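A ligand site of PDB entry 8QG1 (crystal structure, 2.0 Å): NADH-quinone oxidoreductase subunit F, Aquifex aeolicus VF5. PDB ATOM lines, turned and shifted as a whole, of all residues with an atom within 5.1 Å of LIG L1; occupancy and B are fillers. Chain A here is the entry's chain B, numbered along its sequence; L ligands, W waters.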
ATOM      1  N   GLY A  65       8.063   0.909   3.296  1.00  0.00           N
ATOM      2  CA  GLY A  65       9.160   1.324   2.430  1.00  0.00           C
ATOM      3  C   GLY A  65       9.228   2.839   2.273  1.00  0.00           C
ATOM      4  O   GLY A  65       8.213   3.500   2.056  1.00  0.00           O
ATOM      5  N   ARG A  66      10.450   3.368   2.371  1.00  0.00           N
ATOM      6  CA  ARG A  66      10.707   4.801   2.252  1.00  0.00           C
ATOM      7  C   ARG A  66      11.342   5.120   0.893  1.00  0.00           C
ATOM      8  O   ARG A  66      11.794   6.238   0.666  1.00  0.00           O
ATOM      9  CB  ARG A  66      11.652   5.241   3.375  1.00  0.00           C
ATOM     10  CG  ARG A  66      11.170   4.937   4.782  1.00  0.00           C
ATOM     11  CD  ARG A  66       9.924   5.709   5.174  1.00  0.00           C
ATOM     12  NE  ARG A  66       9.781   5.788   6.621  1.00  0.00           N
ATOM     13  CZ  ARG A  66       8.729   5.397   7.317  1.00  0.00           C
ATOM     14  NH1 ARG A  66       8.642   5.682   8.602  1.00  0.00           N
ATOM     15  NH2 ARG A  66       7.734   4.754   6.720  1.00  0.00           N
ATOM     16  N   GLY A  67      11.358   4.131  -0.014  1.00  0.00           N
ATOM     17  CA  GLY A  67      12.019   4.282  -1.296  1.00  0.00           C
ATOM     18  C   GLY A  67      11.051   4.727  -2.406  1.00  0.00           C
ATOM     19  O   GLY A  67      11.467   4.894  -3.545  1.00  0.00           O
ATOM     20  N   GLY A  68       9.757   4.885  -2.052  1.00  0.00           N
ATOM     21  CA  GLY A  68       8.815   5.496  -2.964  1.00  0.00           C
ATOM     22  C   GLY A  68       7.448   4.816  -3.004  1.00  0.00           C
ATOM     23  O   GLY A  68       6.454   5.499  -3.243  1.00  0.00           O
ATOM     24  N   ALA A  69       7.393   3.490  -2.800  1.00  0.00           N
ATOM     25  CA  ALA A  69       6.180   2.696  -3.050  1.00  0.00           C
ATOM     26  C   ALA A  69       5.448   2.321  -1.755  1.00  0.00           C
ATOM     27  O   ALA A  69       4.329   1.812  -1.824  1.00  0.00           O
ATOM     28  CB  ALA A  69       6.527   1.464  -3.845  1.00  0.00           C
ATOM     29  N   PHE A  71       5.657  -0.081   0.543  1.00  0.00           N
ATOM     30  CA  PHE A  71       5.281  -1.453   0.821  1.00  0.00           C
ATOM     31  C   PHE A  71       5.649  -1.823   2.260  1.00  0.00           C
ATOM     32  O   PHE A  71       6.716  -1.445   2.731  1.00  0.00           O
ATOM     33  CB  PHE A  71       5.903  -2.407  -0.210  1.00  0.00           C
ATOM     34  CG  PHE A  71       5.423  -3.836  -0.112  1.00  0.00           C
ATOM     35  CD1 PHE A  71       6.027  -4.728   0.754  1.00  0.00           C
ATOM     36  CD2 PHE A  71       4.334  -4.275  -0.840  1.00  0.00           C
ATOM     37  CE1 PHE A  71       5.583  -6.041   0.866  1.00  0.00           C
ATOM     38  CE2 PHE A  71       3.867  -5.572  -0.725  1.00  0.00           C
ATOM     39  CZ  PHE A  71       4.496  -6.460   0.123  1.00  0.00           C
ATOM     40  N   LYS A  76       7.319  -7.768   3.544  1.00  0.00           N
ATOM     41  CA  LYS A  76       8.304  -8.067   2.523  1.00  0.00           C
ATOM     42  C   LYS A  76       9.256  -9.127   3.061  1.00  0.00           C
ATOM     43  O   LYS A  76       9.565 -10.091   2.361  1.00  0.00           O
ATOM     44  CB  LYS A  76       9.061  -6.819   2.067  1.00  0.00           C
ATOM     45  CG  LYS A  76       9.910  -7.021   0.827  1.00  0.00           C
ATOM     46  CD  LYS A  76      10.829  -5.872   0.476  1.00  0.00           C
ATOM     47  CE  LYS A  76      10.105  -4.585   0.137  1.00  0.00           C
ATOM     48  NZ  LYS A  76      11.045  -3.552  -0.374  1.00  0.00           N
ATOM     49  N   ASN A  92      19.392  -0.265  -0.894  1.00  0.00           N
ATOM     50  CA  ASN A  92      19.279   0.543  -2.099  1.00  0.00           C
ATOM     51  C   ASN A  92      19.680   1.975  -1.767  1.00  0.00           C
ATOM     52  O   ASN A  92      18.904   2.720  -1.176  1.00  0.00           O
ATOM     53  CB  ASN A  92      17.853   0.455  -2.675  1.00  0.00           C
ATOM     54  CG  ASN A  92      17.698   1.124  -4.015  1.00  0.00           C
ATOM     55  OD1 ASN A  92      18.524   1.951  -4.409  1.00  0.00           O
ATOM     56  ND2 ASN A  92      16.638   0.779  -4.732  1.00  0.00           N
ATOM     57  N   ASP A  94      20.694   4.168  -4.311  1.00  0.00           N
ATOM     58  CA  ASP A  94      20.876   4.725  -5.637  1.00  0.00           C
ATOM     59  C   ASP A  94      20.296   6.147  -5.763  1.00  0.00           C
ATOM     60  O   ASP A  94      20.651   6.859  -6.686  1.00  0.00           O
ATOM     61  CB  ASP A  94      20.293   3.836  -6.735  1.00  0.00           C
ATOM     62  CG  ASP A  94      20.921   4.155  -8.082  1.00  0.00           C
ATOM     63  OD1 ASP A  94      22.146   3.966  -8.215  1.00  0.00           O
ATOM     64  OD2 ASP A  94      20.203   4.649  -8.967  1.00  0.00           O
ATOM     65  N   GLU A  95      19.414   6.539  -4.828  1.00  0.00           N
ATOM     66  CA  GLU A  95      18.831   7.875  -4.728  1.00  0.00           C
ATOM     67  C   GLU A  95      19.267   8.834  -5.844  1.00  0.00           C
ATOM     68  O   GLU A  95      20.262   9.543  -5.712  1.00  0.00           O
ATOM     69  CB  GLU A  95      19.192   8.482  -3.367  1.00  0.00           C
ATOM     70  CG  GLU A  95      18.569   9.850  -3.145  1.00  0.00           C
ATOM     71  CD  GLU A  95      18.722  10.353  -1.729  1.00  0.00           C
ATOM     72  OE1 GLU A  95      19.865  10.682  -1.344  1.00  0.00           O
ATOM     73  OE2 GLU A  95      17.686  10.400  -0.995  1.00  0.00           O
ATOM     74  N   SER A  96      18.450   8.907  -6.906  1.00  0.00           N
ATOM     75  CA  SER A  96      18.789   9.674  -8.095  1.00  0.00           C
ATOM     76  C   SER A  96      17.591  10.448  -8.661  1.00  0.00           C
ATOM     77  O   SER A  96      17.746  11.136  -9.680  1.00  0.00           O
ATOM     78  CB  SER A  96      19.371   8.778  -9.150  1.00  0.00           C
ATOM     79  OG  SER A  96      20.704   8.404  -8.819  1.00  0.00           O
ATOM     80  N   ASP A 103      18.532  10.294   1.642  1.00  0.00           N
ATOM     81  CA  ASP A 103      19.285   9.088   1.985  1.00  0.00           C
ATOM     82  C   ASP A 103      20.753   9.432   2.227  1.00  0.00           C
ATOM     83  O   ASP A 103      21.396   8.843   3.093  1.00  0.00           O
ATOM     84  CB  ASP A 103      19.176   8.008   0.912  1.00  0.00           C
ATOM     85  CG  ASP A 103      17.788   7.424   0.737  1.00  0.00           C
ATOM     86  OD1 ASP A 103      16.936   7.668   1.614  1.00  0.00           O
ATOM     87  OD2 ASP A 103      17.571   6.718  -0.257  1.00  0.00           O
ATOM     88  N   TYR A 180      19.812   6.156 -13.519  1.00  0.00           N
ATOM     89  CA  TYR A 180      18.702   6.284 -12.580  1.00  0.00           C
ATOM     90  C   TYR A 180      17.946   4.959 -12.448  1.00  0.00           C
ATOM     91  O   TYR A 180      17.451   4.647 -11.368  1.00  0.00           O
ATOM     92  CB  TYR A 180      17.730   7.386 -13.026  1.00  0.00           C
ATOM     93  CG  TYR A 180      16.403   7.411 -12.308  1.00  0.00           C
ATOM     94  CD1 TYR A 180      16.309   7.725 -10.965  1.00  0.00           C
ATOM     95  CD2 TYR A 180      15.230   7.118 -12.982  1.00  0.00           C
ATOM     96  CE1 TYR A 180      15.093   7.735 -10.308  1.00  0.00           C
ATOM     97  CE2 TYR A 180      14.001   7.124 -12.332  1.00  0.00           C
ATOM     98  CZ  TYR A 180      13.928   7.432 -10.993  1.00  0.00           C
ATOM     99  OH  TYR A 180      12.706   7.426 -10.363  1.00  0.00           O
ATOM    100  N   ILE A 181      17.870   4.205 -13.558  1.00  0.00           N
ATOM    101  CA  ILE A 181      17.058   2.995 -13.587  1.00  0.00           C
ATOM    102  C   ILE A 181      17.636   1.934 -12.639  1.00  0.00           C
ATOM    103  O   ILE A 181      16.926   1.006 -12.276  1.00  0.00           O
ATOM    104  CB  ILE A 181      16.892   2.424 -15.016  1.00  0.00           C
ATOM    105  CG1 ILE A 181      15.777   1.384 -15.084  1.00  0.00           C
ATOM    106  CG2 ILE A 181      18.202   1.852 -15.551  1.00  0.00           C
ATOM    107  CD1 ILE A 181      14.444   1.879 -14.598  1.00  0.00           C
ATOM    108  N   GLY A 183      18.160   2.243  -9.678  1.00  0.00           N
ATOM    109  CA  GLY A 183      17.425   2.330  -8.421  1.00  0.00           C
ATOM    110  C   GLY A 183      16.173   1.450  -8.392  1.00  0.00           C
ATOM    111  O   GLY A 183      15.663   1.144  -7.320  1.00  0.00           O
ATOM    112  N   GLU A 184      15.667   1.078  -9.576  1.00  0.00           N
ATOM    113  CA  GLU A 184      14.610   0.078  -9.671  1.00  0.00           C
ATOM    114  C   GLU A 184      15.223  -1.241  -9.237  1.00  0.00           C
ATOM    115  O   GLU A 184      16.328  -1.575  -9.674  1.00  0.00           O
ATOM    116  CB  GLU A 184      14.035   0.045 -11.089  1.00  0.00           C
ATOM    117  CG  GLU A 184      12.680  -0.656 -11.202  1.00  0.00           C
ATOM    118  CD  GLU A 184      12.680  -2.175 -11.224  1.00  0.00           C
ATOM    119  OE1 GLU A 184      13.767  -2.769 -11.388  1.00  0.00           O
ATOM    120  OE2 GLU A 184      11.594  -2.758 -11.049  1.00  0.00           O
ATOM    121  N   GLU A 185      14.523  -1.984  -8.365  1.00  0.00           N
ATOM    122  CA  GLU A 185      15.164  -3.013  -7.562  1.00  0.00           C
ATOM    123  C   GLU A 185      15.735  -4.139  -8.428  1.00  0.00           C
ATOM    124  O   GLU A 185      16.779  -4.690  -8.096  1.00  0.00           O
ATOM    125  CB  GLU A 185      14.219  -3.574  -6.491  1.00  0.00           C
ATOM    126  CG  GLU A 185      12.898  -4.100  -7.032  1.00  0.00           C
ATOM    127  CD  GLU A 185      11.973  -4.703  -5.989  1.00  0.00           C
ATOM    128  OE1 GLU A 185      12.337  -4.715  -4.775  1.00  0.00           O
ATOM    129  OE2 GLU A 185      10.890  -5.168  -6.401  1.00  0.00           O
ATOM    130  N   VAL A 218      15.238  -6.188  -1.090  1.00  0.00           N
ATOM    131  CA  VAL A 218      15.762  -4.863  -1.368  1.00  0.00           C
ATOM    132  C   VAL A 218      14.996  -3.860  -0.511  1.00  0.00           C
ATOM    133  O   VAL A 218      13.768  -3.835  -0.540  1.00  0.00           O
ATOM    134  CB  VAL A 218      15.656  -4.489  -2.854  1.00  0.00           C
ATOM    135  CG1 VAL A 218      16.264  -3.119  -3.114  1.00  0.00           C
ATOM    136  CG2 VAL A 218      16.266  -5.549  -3.758  1.00  0.00           C
ATOM    137  N   ASN A 219      15.737  -3.053   0.250  1.00  0.00           N
ATOM    138  CA  ASN A 219      15.160  -2.000   1.061  1.00  0.00           C
ATOM    139  C   ASN A 219      15.947  -0.709   0.875  1.00  0.00           C
ATOM    140  O   ASN A 219      17.168  -0.736   0.660  1.00  0.00           O
ATOM    141  CB  ASN A 219      15.037  -2.370   2.539  1.00  0.00           C
ATOM    142  CG  ASN A 219      13.764  -3.127   2.887  1.00  0.00           C
ATOM    143  OD1 ASN A 219      13.822  -4.175   3.514  1.00  0.00           O
ATOM    144  ND2 ASN A 219      12.615  -2.575   2.532  1.00  0.00           N
ATOM    145  N   ASN A 220      15.223   0.408   0.942  1.00  0.00           N
ATOM    146  CA  ASN A 220      15.785   1.742   0.843  1.00  0.00           C
ATOM    147  C   ASN A 220      16.577   2.054   2.108  1.00  0.00           C
ATOM    148  O   ASN A 220      16.243   1.550   3.177  1.00  0.00           O
ATOM    149  CB  ASN A 220      14.659   2.762   0.624  1.00  0.00           C
ATOM    150  CG  ASN A 220      15.088   4.204   0.731  1.00  0.00           C
ATOM    151  OD1 ASN A 220      14.856   4.846   1.756  1.00  0.00           O
ATOM    152  ND2 ASN A 220      15.756   4.702  -0.307  1.00  0.00           N
ATOM    153  N   VAL A 221      17.604   2.901   1.970  1.00  0.00           N
ATOM    154  CA  VAL A 221      18.431   3.412   3.068  1.00  0.00           C
ATOM    155  C   VAL A 221      17.574   3.843   4.254  1.00  0.00           C
ATOM    156  O   VAL A 221      17.799   3.396   5.391  1.00  0.00           O
ATOM    157  CB  VAL A 221      19.309   4.578   2.575  1.00  0.00           C
ATOM    158  CG1 VAL A 221      19.913   5.358   3.737  1.00  0.00           C
ATOM    159  CG2 VAL A 221      20.392   4.135   1.604  1.00  0.00           C
ATOM    160  N   THR A 223      14.433   3.327   5.051  1.00  0.00           N
ATOM    161  CA  THR A 223      13.717   2.194   5.628  1.00  0.00           C
ATOM    162  C   THR A 223      14.599   1.472   6.649  1.00  0.00           C
ATOM    163  O   THR A 223      14.187   1.234   7.793  1.00  0.00           O
ATOM    164  CB  THR A 223      13.274   1.189   4.560  1.00  0.00           C
ATOM    165  OG1 THR A 223      12.689   1.875   3.449  1.00  0.00           O
ATOM    166  CG2 THR A 223      12.311   0.155   5.099  1.00  0.00           C
ATOM    167  N   CYS A 393       8.450  -1.946 -15.968  1.00  0.00           N
ATOM    168  CA  CYS A 393       8.815  -1.342 -14.692  1.00  0.00           C
ATOM    169  C   CYS A 393       8.133   0.012 -14.525  1.00  0.00           C
ATOM    170  O   CYS A 393       7.513   0.532 -15.456  1.00  0.00           O
ATOM    171  CB  CYS A 393      10.329  -1.214 -14.496  1.00  0.00           C
ATOM    172  SG  CYS A 393      11.072   0.350 -15.036  1.00  0.00           S
ATOM    173  N   GLY A 394       8.259   0.566 -13.316  1.00  0.00           N
ATOM    174  CA  GLY A 394       7.504   1.736 -12.900  1.00  0.00           C
ATOM    175  C   GLY A 394       7.894   3.012 -13.630  1.00  0.00           C
ATOM    176  O   GLY A 394       7.113   3.957 -13.632  1.00  0.00           O
ATOM    177  N   LEU A 395       9.093   3.046 -14.249  1.00  0.00           N
ATOM    178  CA  LEU A 395       9.504   4.248 -14.956  1.00  0.00           C
ATOM    179  C   LEU A 395       8.525   4.528 -16.097  1.00  0.00           C
ATOM    180  O   LEU A 395       7.969   5.630 -16.172  1.00  0.00           O
ATOM    181  CB  LEU A 395      10.950   4.102 -15.454  1.00  0.00           C
ATOM    182  CG  LEU A 395      11.581   5.385 -16.010  1.00  0.00           C
ATOM    183  CD1 LEU A 395      13.092   5.378 -15.801  1.00  0.00           C
ATOM    184  CD2 LEU A 395      11.264   5.571 -17.494  1.00  0.00           C
HETATM  185  N1  LIG L   1      14.117   2.769  -4.350  1.00  0.00           N
HETATM  186  C1  LIG L   1      15.176   3.251  -3.624  1.00  0.00           C
HETATM  187  O1  LIG L   1      15.401   2.873  -2.451  1.00  0.00           O
HETATM  188  N2  LIG L   1      16.092   4.115  -4.236  1.00  0.00           N
HETATM  189  C2  LIG L   1      16.068   4.528  -5.552  1.00  0.00           C
HETATM  190  O2  LIG L   1      16.965   5.263  -5.977  1.00  0.00           O
HETATM  191  C3  LIG L   1      14.946   4.000  -6.333  1.00  0.00           C
HETATM  192  N3  LIG L   1      14.862   4.302  -7.605  1.00  0.00           N
HETATM  193  C4  LIG L   1      13.812   3.757  -8.339  1.00  0.00           C
HETATM  194  C5  LIG L   1      13.729   4.054  -9.705  1.00  0.00           C
HETATM  195  C6  LIG L   1      12.692   3.536 -10.482  1.00  0.00           C
HETATM  196  C7  LIG L   1      12.615   3.900 -11.953  1.00  0.00           C
HETATM  197  C8  LIG L   1      11.728   2.709  -9.897  1.00  0.00           C
HETATM  198  C9  LIG L   1      10.546   2.223 -10.704  1.00  0.00           C
HETATM  199  C10 LIG L   1      11.805   2.408  -8.550  1.00  0.00           C
HETATM  200  C11 LIG L   1      12.836   2.926  -7.760  1.00  0.00           C
HETATM  201  N4  LIG L   1      12.969   2.624  -6.375  1.00  0.00           N
HETATM  202  C12 LIG L   1      14.010   3.127  -5.628  1.00  0.00           C
HETATM  203  C13 LIG L   1      12.035   1.701  -5.722  1.00  0.00           C
HETATM  204  C14 LIG L   1      12.637   0.307  -5.706  1.00  0.00           C
HETATM  205  O3  LIG L   1      12.336  -0.366  -6.929  1.00  0.00           O
HETATM  206  C15 LIG L   1      12.099  -0.487  -4.515  1.00  0.00           C
HETATM  207  O4  LIG L   1      10.678  -0.337  -4.444  1.00  0.00           O
HETATM  208  C16 LIG L   1      12.697  -0.074  -3.165  1.00  0.00           C
HETATM  209  O5  LIG L   1      14.120   0.007  -3.230  1.00  0.00           O
HETATM  210  C17 LIG L   1      12.286  -1.031  -2.069  1.00  0.00           C
HETATM  211  O6  LIG L   1      12.722  -0.542  -0.775  1.00  0.00           O
HETATM  212  P1  LIG L   1      11.602  -0.001   0.268  1.00  0.00           P
HETATM  213  O7  LIG L   1      12.380   0.092   1.559  1.00  0.00           O
HETATM  214  O8  LIG L   1      11.119   1.335  -0.251  1.00  0.00           O
HETATM  215  O9  LIG L   1      10.485  -1.026   0.358  1.00  0.00           O
HETATM  216  N1  LG2 L   2       5.110  -9.636  -3.165  1.00  0.00           N
HETATM  217  C1  LG2 L   2       6.321  -9.314  -2.680  1.00  0.00           C
HETATM  218  N2  LG2 L   2       6.940  -8.128  -2.695  1.00  0.00           N
HETATM  219  C2  LG2 L   2       6.185  -7.197  -3.290  1.00  0.00           C
HETATM  220  C3  LG2 L   2       4.916  -7.376  -3.836  1.00  0.00           C
HETATM  221  C4  LG2 L   2       4.369  -8.670  -3.763  1.00  0.00           C
HETATM  222  N3  LG2 L   2       3.186  -9.010  -4.273  1.00  0.00           N
HETATM  223  N4  LG2 L   2       4.429  -6.186  -4.350  1.00  0.00           N
HETATM  224  C5  LG2 L   2       5.390  -5.321  -4.108  1.00  0.00           C
HETATM  225  N5  LG2 L   2       6.484  -5.869  -3.471  1.00  0.00           N
HETATM  226  C6  LG2 L   2       7.714  -5.181  -3.135  1.00  0.00           C
HETATM  227  C7  LG2 L   2       8.650  -4.957  -4.324  1.00  0.00           C
HETATM  228  O1  LG2 L   2       9.531  -6.075  -4.501  1.00  0.00           O
HETATM  229  C8  LG2 L   2       9.383  -3.676  -3.892  1.00  0.00           C
HETATM  230  O2  LG2 L   2      10.535  -3.952  -3.092  1.00  0.00           O
HETATM  231  O3  LG2 L   2       7.388  -3.899  -2.627  1.00  0.00           O
HETATM  232  C9  LG2 L   2       8.307  -2.901  -3.123  1.00  0.00           C
HETATM  233  C10 LG2 L   2       7.548  -1.881  -3.932  1.00  0.00           C
HETATM  234  O4  LG2 L   2       7.119  -2.514  -5.160  1.00  0.00           O
HETATM  235  P1  LG2 L   2       6.286  -1.782  -6.316  1.00  0.00           P
HETATM  236  O5  LG2 L   2       4.963  -1.370  -5.781  1.00  0.00           O
HETATM  237  O6  LG2 L   2       6.307  -2.718  -7.463  1.00  0.00           O
HETATM  238  O7  LG2 L   2       7.143  -0.476  -6.634  1.00  0.00           O
HETATM  239  P2  LG2 L   2       8.508  -0.223  -7.431  1.00  0.00           P
HETATM  240  O8  LG2 L   2       8.285  -0.467  -8.880  1.00  0.00           O
HETATM  241  O9  LG2 L   2       9.638  -0.902  -6.762  1.00  0.00           O
HETATM  242  O10 LG2 L   2       8.760   1.335  -7.183  1.00  0.00           O
HETATM  243  C11 LG2 L   2       7.805   2.331  -7.607  1.00  0.00           C
HETATM  244  O11 LG2 L   2       9.302   4.238  -7.544  1.00  0.00           O
HETATM  245  O12 LG2 L   2       8.737   5.562  -9.407  1.00  0.00           O
HETATM  246  C12 LG2 L   2       9.023   5.551  -8.010  1.00  0.00           C
HETATM  247  O13 LG2 L   2       8.075   6.480  -5.935  1.00  0.00           O
HETATM  248  C13 LG2 L   2       7.776   5.992  -7.237  1.00  0.00           C
HETATM  249  O14 LG2 L   2       6.106   4.679  -6.034  1.00  0.00           O
HETATM  250  C14 LG2 L   2       6.995   4.688  -7.135  1.00  0.00           C
HETATM  251  C15 LG2 L   2       8.107   3.656  -6.962  1.00  0.00           C
HETATM  252  O   HOH W   1      15.656   7.766  -6.539  1.00  0.00           O
HETATM  253  O   HOH W   2      12.801   6.184  -5.307  1.00  0.00           O
HETATM  254  O   HOH W   3       9.408  -2.178   2.728  1.00  0.00           O
HETATM  255  O   HOH W   4      17.811   5.650  -8.690  1.00  0.00           O
HETATM  256  O   HOH W   5      18.168   5.194  -2.307  1.00  0.00           O
HETATM  257  O   HOH W   6       9.670   1.532  -2.464  1.00  0.00           O
HETATM  258  O   HOH W   7       8.226  -0.290  -0.785  1.00  0.00           O
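The backbone NH of Arg 66 sits at hydrogen-bond distance from the side-chain hydroxyl of Thr 223 (2.9 Å). The side-chain amide nitrogen (ND2) of Asn 219 lies close to the side-chain amino group (NZ) of Lys 76 (3.4 Å). The side-chain amide nitrogen (ND2) of Asn 220 is in hydrogen-bond range of the side-chain carboxylate (OD2) of Asp 103 (2.7 Å). The backbone carbonyl oxygen of Asn 219 is in hydrogen-bond range of the backbone NH of Asn 92 (2.8 Å). O of Gly 183 sits at hydrogen-bond distance from ND2 of Asn 92. The side-chain amide oxygen (OD1) of Asn 92 sits at hydrogen-bond distance from the backbone NH (N) of Asp 94 (3.1 Å). N of Gly 65 sits at hydrogen-bond distance from O of Phe 71, 2.8 Å away. The side-chain hydroxyl (OG) of Ser 96 lies within hydrogen-bond range of the backbone carbonyl oxygen (O) of Asp 94, 2.6 Å away.
O of Gly 183 lies close to N4 of LIG L1, at 3.2 Å. An oxygen (O6) of LIG L1 lies close to the backbone carbonyl oxygen (O) of Val 218 (3.5 Å). Residues that only touch LIG L1: Gly 65 (3.3 Å), Asp 94 (3.5 Å), Tyr 180 (3.5 Å), Ile 181 (3.8 Å), Glu 184 (3.5 Å), Gly 394 (3.8 Å) and Leu 395 (3.9 Å). Hydrophobic or aromatic side chains that line LIG L1: Tyr 180, Ile 181, Val 218 and Leu 395. 18 residues have an atom within 4 Å of LIG L1: Gly 65, Arg 66, Gly 67, Lys 76, Asn 92, Asp 94, Glu 95, Tyr 180, Ile 181, Gly 183, Glu 184, Glu 185, Val 218, Asn 219, Asn 220, Thr 223, Gly 394 and Leu 395.
An oxygen (O4) of LIG L1 sits at hydrogen-bond distance from an oxygen (O9) of LG2 L2 (2.6 Å).
Water W7 bridges an oxygen (O9) of LIG L1 (2.6 Å) and the backbone NH of Phe 71 (2.9 Å). Water W6 lies within hydrogen-bond range of an oxygen (O8) of LIG L1 (2.7 Å), the backbone NH of Ala 69 (3.0 Å) and the backbone NH of Gly 68 (3.4 Å). Water W3 lies within hydrogen-bond range of O of Phe 71 (2.8 Å), O9 of LIG L1 (2.8 Å), ND2 of Asn 219 (3.2 Å) and N of Gly 65 (3.4 Å). Water W1 bridges an oxygen (O2) of LIG L1 (2.9 Å) and the backbone NH (N) of Ser 96 (3.0 Å).
An oxygen (O7) of LIG L1 sits at hydrogen-bond distance from the side-chain hydroxyl (OG1) of Thr 223, 2.6 Å away. NZ of Lys 76 lies within salt-bridge range of O9 of LIG L1. O8 of LIG L1 sits at hydrogen-bond distance from N of Gly 67 (2.8 Å). The backbone NH (N) of Asn 220 sits at hydrogen-bond distance from an oxygen (O7) of LIG L1. The side-chain amide nitrogen of Asn 220 lies within hydrogen-bond range of an oxygen (O1) of LIG L1 (2.8 Å). The side-chain amide nitrogen (ND2) of Asn 219 sits at hydrogen-bond distance from an oxygen (O7) of LIG L1, at 2.8 Å. The backbone NH of Glu 95 lies within hydrogen-bond range of an oxygen (O2) of LIG L1 (3.0 Å). O5 of LIG L1 sits at hydrogen-bond distance from ND2 of Asn 92 (3.0 Å). The backbone NH (N) of Glu 185 sits at hydrogen-bond distance from an oxygen (O3) of LIG L1 (3.1 Å). The backbone NH of Arg 66 lies within hydrogen-bond range of an oxygen (O8) of LIG L1, at 3.4 Å. The side-chain amino group (NZ) of Lys 76 sits at hydrogen-bond distance from an oxygen (O2) of LG2 L2, at 2.8 Å. The side-chain carboxylate (OE2) of Glu 185 is in hydrogen-bond range of an oxygen (O1) of LG2 L2 (2.5 Å). The backbone carbonyl oxygen of Gly 68 sits at hydrogen-bond distance from an oxygen (O14) of LG2 L2 (2.9 Å).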
